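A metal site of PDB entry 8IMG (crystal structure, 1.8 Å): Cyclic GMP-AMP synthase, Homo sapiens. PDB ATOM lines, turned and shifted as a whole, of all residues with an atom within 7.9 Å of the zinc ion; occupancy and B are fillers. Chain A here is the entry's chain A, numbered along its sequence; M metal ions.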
ATOM      1  N   LEU A 231     -20.434 -36.554  -4.970  1.00  0.00           N
ATOM      2  CA  LEU A 231     -21.168 -35.602  -4.125  1.00  0.00           C
ATOM      3  C   LEU A 231     -20.549 -35.464  -2.736  1.00  0.00           C
ATOM      4  O   LEU A 231     -20.551 -34.358  -2.164  1.00  0.00           O
ATOM      5  CB  LEU A 231     -22.631 -36.049  -4.013  1.00  0.00           C
ATOM      6  CG  LEU A 231     -23.562 -35.005  -3.396  1.00  0.00           C
ATOM      7  CD1 LEU A 231     -23.704 -33.826  -4.362  1.00  0.00           C
ATOM      8  CD2 LEU A 231     -24.934 -35.615  -3.046  1.00  0.00           C
ATOM      9  N   ASN A 232     -20.027 -36.561  -2.182  1.00  0.00           N
ATOM     10  CA  ASN A 232     -19.415 -36.553  -0.864  1.00  0.00           C
ATOM     11  C   ASN A 232     -17.933 -36.223  -0.908  1.00  0.00           C
ATOM     12  O   ASN A 232     -17.340 -35.994   0.151  1.00  0.00           O
ATOM     13  CB  ASN A 232     -19.555 -37.908  -0.179  1.00  0.00           C
ATOM     14  CG  ASN A 232     -20.964 -38.196   0.275  1.00  0.00           C
ATOM     15  OD1 ASN A 232     -21.709 -37.288   0.649  1.00  0.00           O
ATOM     16  ND2 ASN A 232     -21.317 -39.472   0.312  1.00  0.00           N
ATOM     17  N   ASN A 233     -17.319 -36.270  -2.072  1.00  0.00           N
ATOM     18  CA  ASN A 233     -15.925 -35.861  -2.225  1.00  0.00           C
ATOM     19  C   ASN A 233     -15.902 -34.875  -3.394  1.00  0.00           C
ATOM     20  O   ASN A 233     -15.464 -35.194  -4.510  1.00  0.00           O
ATOM     21  CB  ASN A 233     -15.024 -37.076  -2.453  1.00  0.00           C
ATOM     22  CG  ASN A 233     -13.550 -36.737  -2.277  1.00  0.00           C
ATOM     23  OD1 ASN A 233     -13.202 -35.606  -1.966  1.00  0.00           O
ATOM     24  ND2 ASN A 233     -12.697 -37.729  -2.452  1.00  0.00           N
ATOM     25  N   HIS A 234     -16.351 -33.647  -3.127  1.00  0.00           N
ATOM     26  CA  HIS A 234     -16.924 -32.790  -4.155  1.00  0.00           C
ATOM     27  C   HIS A 234     -16.091 -31.554  -4.485  1.00  0.00           C
ATOM     28  O   HIS A 234     -16.482 -30.815  -5.395  1.00  0.00           O
ATOM     29  CB  HIS A 234     -18.311 -32.297  -3.702  1.00  0.00           C
ATOM     30  CG  HIS A 234     -18.270 -31.513  -2.423  1.00  0.00           C
ATOM     31  ND1 HIS A 234     -18.894 -31.932  -1.275  1.00  0.00           N
ATOM     32  CD2 HIS A 234     -17.659 -30.342  -2.113  1.00  0.00           C
ATOM     33  CE1 HIS A 234     -18.692 -31.044  -0.306  1.00  0.00           C
ATOM     34  NE2 HIS A 234     -17.934 -30.077  -0.799  1.00  0.00           N
ATOM     35  N   GLY A 235     -15.006 -31.297  -3.768  1.00  0.00           N
ATOM     36  CA  GLY A 235     -14.239 -30.090  -3.968  1.00  0.00           C
ATOM     37  C   GLY A 235     -13.075 -30.300  -4.906  1.00  0.00           C
ATOM     38  O   GLY A 235     -12.602 -31.410  -5.111  1.00  0.00           O
ATOM     39  N   LYS A 236     -12.640 -29.207  -5.526  1.00  0.00           N
ATOM     40  CA  LYS A 236     -11.315 -29.238  -6.124  1.00  0.00           C
ATOM     41  C   LYS A 236     -10.256 -29.438  -5.041  1.00  0.00           C
ATOM     42  O   LYS A 236      -9.323 -30.231  -5.215  1.00  0.00           O
ATOM     43  CB  LYS A 236     -11.050 -27.967  -6.921  1.00  0.00           C
ATOM     44  CG  LYS A 236      -9.582 -27.894  -7.467  1.00  0.00           C
ATOM     45  CD  LYS A 236      -9.323 -26.752  -8.476  1.00  0.00           C
ATOM     46  CE  LYS A 236     -10.032 -26.935  -9.844  1.00  0.00           C
ATOM     47  NZ  LYS A 236      -9.904 -28.330 -10.471  1.00  0.00           N
ATOM     48  N   SER A 237     -10.385 -28.741  -3.922  1.00  0.00           N
ATOM     49  CA  SER A 237      -9.494 -29.020  -2.800  1.00  0.00           C
ATOM     50  C   SER A 237      -9.889 -30.325  -2.123  1.00  0.00           C
ATOM     51  O   SER A 237     -11.058 -30.576  -1.850  1.00  0.00           O
ATOM     52  CB  SER A 237      -9.520 -27.894  -1.777  1.00  0.00           C
ATOM     53  OG  SER A 237      -8.922 -28.320  -0.555  1.00  0.00           O
ATOM     54  N   THR A 239      -9.447 -30.831   0.909  1.00  0.00           N
ATOM     55  CA  THR A 239      -9.965 -30.457   2.216  1.00  0.00           C
ATOM     56  C   THR A 239     -11.196 -29.561   2.123  1.00  0.00           C
ATOM     57  O   THR A 239     -11.565 -28.938   3.132  1.00  0.00           O
ATOM     58  CB  THR A 239      -8.890 -29.791   3.078  1.00  0.00           C
ATOM     59  OG1 THR A 239      -8.102 -28.868   2.305  1.00  0.00           O
ATOM     60  CG2 THR A 239      -7.975 -30.864   3.712  1.00  0.00           C
ATOM     61  N   CYS A 240     -11.851 -29.480   0.957  1.00  0.00           N
ATOM     62  CA  CYS A 240     -13.128 -28.769   0.872  1.00  0.00           C
ATOM     63  C   CYS A 240     -14.070 -29.247   1.961  1.00  0.00           C
ATOM     64  O   CYS A 240     -14.213 -30.444   2.188  1.00  0.00           O
ATOM     65  CB  CYS A 240     -13.770 -28.975  -0.508  1.00  0.00           C
ATOM     66  SG  CYS A 240     -15.136 -27.825  -0.848  1.00  0.00           S
ATOM     67  N   CYS A 241     -14.640 -28.286   2.675  1.00  0.00           N
ATOM     68  CA  CYS A 241     -15.591 -28.446   3.788  1.00  0.00           C
ATOM     69  C   CYS A 241     -14.967 -29.101   5.018  1.00  0.00           C
ATOM     70  O   CYS A 241     -15.699 -29.436   5.958  1.00  0.00           O
ATOM     71  CB  CYS A 241     -16.852 -29.191   3.326  1.00  0.00           C
ATOM     72  SG  CYS A 241     -17.906 -28.136   2.223  1.00  0.00           S
ATOM     73  N   GLU A 242     -13.650 -29.250   5.079  1.00  0.00           N
ATOM     74  CA  GLU A 242     -13.056 -29.899   6.249  1.00  0.00           C
ATOM     75  C   GLU A 242     -12.577 -28.903   7.288  1.00  0.00           C
ATOM     76  O   GLU A 242     -12.118 -29.300   8.371  1.00  0.00           O
ATOM     77  CB  GLU A 242     -11.895 -30.816   5.802  1.00  0.00           C
ATOM     78  CG  GLU A 242     -12.420 -32.113   5.230  1.00  0.00           C
ATOM     79  CD  GLU A 242     -11.368 -33.187   5.183  1.00  0.00           C
ATOM     80  OE1 GLU A 242     -11.665 -34.316   4.722  1.00  0.00           O
ATOM     81  OE2 GLU A 242     -10.214 -32.879   5.601  1.00  0.00           O
ATOM     82  N   GLU A 246     -12.692 -23.477   4.250  1.00  0.00           N
ATOM     83  CA  GLU A 246     -13.040 -24.109   2.974  1.00  0.00           C
ATOM     84  C   GLU A 246     -14.480 -24.589   2.946  1.00  0.00           C
ATOM     85  O   GLU A 246     -14.797 -25.497   2.177  1.00  0.00           O
ATOM     86  CB  GLU A 246     -12.099 -25.270   2.666  1.00  0.00           C
ATOM     87  CG  GLU A 246     -10.603 -24.872   2.683  1.00  0.00           C
ATOM     88  CD  GLU A 246      -9.689 -25.954   2.136  1.00  0.00           C
ATOM     89  OE1 GLU A 246      -9.830 -26.362   0.952  1.00  0.00           O
ATOM     90  OE2 GLU A 246      -8.845 -26.455   2.916  1.00  0.00           O
ATOM     91  N   LYS A 247     -15.356 -24.048   3.797  1.00  0.00           N
ATOM     92  CA  LYS A 247     -16.761 -24.453   3.719  1.00  0.00           C
ATOM     93  C   LYS A 247     -17.356 -23.955   2.408  1.00  0.00           C
ATOM     94  O   LYS A 247     -17.265 -22.757   2.091  1.00  0.00           O
ATOM     95  CB  LYS A 247     -17.553 -23.912   4.900  1.00  0.00           C
ATOM     96  CG  LYS A 247     -17.109 -24.452   6.261  1.00  0.00           C
ATOM     97  CD  LYS A 247     -17.352 -25.944   6.386  1.00  0.00           C
ATOM     98  CE  LYS A 247     -17.139 -26.419   7.819  1.00  0.00           C
ATOM     99  NZ  LYS A 247     -17.197 -27.907   7.933  1.00  0.00           N
ATOM    100  N   CYS A 248     -17.928 -24.864   1.620  1.00  0.00           N
ATOM    101  CA  CYS A 248     -18.628 -24.489   0.378  1.00  0.00           C
ATOM    102  C   CYS A 248     -20.105 -24.851   0.512  1.00  0.00           C
ATOM    103  O   CYS A 248     -20.518 -25.483   1.467  1.00  0.00           O
ATOM    104  CB  CYS A 248     -18.007 -25.170  -0.853  1.00  0.00           C
ATOM    105  SG  CYS A 248     -18.547 -26.915  -1.180  1.00  0.00           S
ATOM    106  N   CYS A 249     -20.911 -24.407  -0.459  1.00  0.00           N
ATOM    107  CA  CYS A 249     -22.350 -24.675  -0.395  1.00  0.00           C
ATOM    108  C   CYS A 249     -22.827 -25.609  -1.493  1.00  0.00           C
ATOM    109  O   CYS A 249     -24.042 -25.662  -1.767  1.00  0.00           O
ATOM    110  CB  CYS A 249     -23.142 -23.366  -0.426  1.00  0.00           C
ATOM    111  SG  CYS A 249     -22.934 -22.413  -1.926  1.00  0.00           S
ATOM    112  N   ARG A 250     -21.939 -26.410  -2.057  1.00  0.00           N
ATOM    113  CA  ARG A 250     -22.333 -27.331  -3.115  1.00  0.00           C
ATOM    114  C   ARG A 250     -23.465 -28.233  -2.650  1.00  0.00           C
ATOM    115  O   ARG A 250     -24.531 -28.292  -3.275  1.00  0.00           O
ATOM    116  CB  ARG A 250     -21.144 -28.162  -3.561  1.00  0.00           C
ATOM    117  CG  ARG A 250     -20.204 -27.440  -4.538  1.00  0.00           C
ATOM    118  CD  ARG A 250     -19.204 -28.447  -5.074  1.00  0.00           C
ATOM    119  NE  ARG A 250     -18.148 -27.872  -5.913  1.00  0.00           N
ATOM    120  CZ  ARG A 250     -17.014 -27.356  -5.473  1.00  0.00           C
ATOM    121  NH1 ARG A 250     -16.767 -27.235  -4.173  1.00  0.00           N
ATOM    122  NH2 ARG A 250     -16.066 -27.014  -6.344  1.00  0.00           N
ATOM    123  N   LYS A 251     -23.254 -28.959  -1.529  1.00  0.00           N
ATOM    124  CA  LYS A 251     -24.257 -29.928  -1.105  1.00  0.00           C
ATOM    125  C   LYS A 251     -25.571 -29.265  -0.720  1.00  0.00           C
ATOM    126  O   LYS A 251     -26.657 -29.802  -1.001  1.00  0.00           O
ATOM    127  CB  LYS A 251     -23.729 -30.758   0.073  1.00  0.00           C
ATOM    128  CG  LYS A 251     -22.583 -31.703  -0.323  1.00  0.00           C
ATOM    129  CD  LYS A 251     -22.004 -32.431   0.886  1.00  0.00           C
ATOM    130  CE  LYS A 251     -22.652 -33.814   1.053  1.00  0.00           C
ATOM    131  NZ  LYS A 251     -21.988 -34.618   2.111  1.00  0.00           N
ATOM    132  N   ASP A 296     -13.584 -24.052  -5.963  1.00  0.00           N
ATOM    133  CA  ASP A 296     -14.311 -24.014  -4.709  1.00  0.00           C
ATOM    134  C   ASP A 296     -14.711 -22.593  -4.331  1.00  0.00           C
ATOM    135  O   ASP A 296     -15.746 -22.385  -3.693  1.00  0.00           O
ATOM    136  CB  ASP A 296     -13.484 -24.616  -3.580  1.00  0.00           C
ATOM    137  CG  ASP A 296     -13.103 -26.034  -3.848  1.00  0.00           C
ATOM    138  OD1 ASP A 296     -13.809 -26.692  -4.652  1.00  0.00           O
ATOM    139  OD2 ASP A 296     -12.061 -26.460  -3.288  1.00  0.00           O
ATOM    140  N   TRP A 299     -18.188 -21.393  -4.819  1.00  0.00           N
ATOM    141  CA  TRP A 299     -19.224 -22.022  -4.011  1.00  0.00           C
ATOM    142  C   TRP A 299     -19.102 -21.613  -2.557  1.00  0.00           C
ATOM    143  O   TRP A 299     -19.460 -22.377  -1.674  1.00  0.00           O
ATOM    144  CB  TRP A 299     -19.159 -23.553  -4.119  1.00  0.00           C
ATOM    145  CG  TRP A 299     -19.414 -24.069  -5.493  1.00  0.00           C
ATOM    146  CD1 TRP A 299     -18.504 -24.330  -6.471  1.00  0.00           C
ATOM    147  CD2 TRP A 299     -20.696 -24.402  -6.021  1.00  0.00           C
ATOM    148  NE1 TRP A 299     -19.148 -24.814  -7.593  1.00  0.00           N
ATOM    149  CE2 TRP A 299     -20.494 -24.877  -7.327  1.00  0.00           C
ATOM    150  CE3 TRP A 299     -21.990 -24.367  -5.494  1.00  0.00           C
ATOM    151  CZ2 TRP A 299     -21.548 -25.283  -8.136  1.00  0.00           C
ATOM    152  CZ3 TRP A 299     -23.040 -24.804  -6.303  1.00  0.00           C
ATOM    153  CH2 TRP A 299     -22.816 -25.222  -7.609  1.00  0.00           C
ATOM    154  N   ARG A 301     -19.718 -20.631   1.008  1.00  0.00           N
ATOM    155  CA  ARG A 301     -20.971 -20.759   1.763  1.00  0.00           C
ATOM    156  C   ARG A 301     -21.595 -19.385   2.021  1.00  0.00           C
ATOM    157  O   ARG A 301     -22.828 -19.285   2.129  1.00  0.00           O
ATOM    158  CB  ARG A 301     -20.715 -21.526   3.073  1.00  0.00           C
ATOM    159  CG  ARG A 301     -21.977 -22.110   3.723  1.00  0.00           C
ATOM    160  CD  ARG A 301     -21.659 -23.172   4.769  1.00  0.00           C
ATOM    161  NE  ARG A 301     -21.207 -24.427   4.172  1.00  0.00           N
ATOM    162  CZ  ARG A 301     -20.942 -25.536   4.849  1.00  0.00           C
ATOM    163  NH1 ARG A 301     -21.064 -25.587   6.169  1.00  0.00           N
ATOM    164  NH2 ARG A 301     -20.517 -26.612   4.194  1.00  0.00           N
HETATM  165 ZN    ZN M   1     -17.185 -28.378   0.037  1.00  0.00          ZN
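O of His 234 lies within hydrogen-bond range of NE of Arg 250 (3.4 Å). ND1 of His 234 lies within hydrogen-bond range of O of Leu 231 (3.1 Å). SG of Cys 240 lies close to NH1 of Arg 250, at 3.8 Å. The side-chain hydroxyl of Ser 237 lies within hydrogen-bond range of the backbone NH of Cys 240 (3.5 Å). N of Cys 241 is in hydrogen-bond range of O of Glu 246 (2.8 Å). NH2 of Arg 301 sits close to SG of Cys 241 (3.6 Å). NH1 of Arg 250 sits close to SG of Cys 248, 3.5 Å away. O of Cys 248 lies within hydrogen-bond range of NH2 of Arg 301.
Of the 20 residues printed, 4 come within 4 Å of the zinc ion. The nearest printed residue that does not touch the zinc ion is Glu 246 (4.3 Å).
The zinc ion is bound by NE2 of His 234, SG of Cys 240, SG of Cys 241 and SG of Cys 248. The zinc ion has four donor atoms within binding distance.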
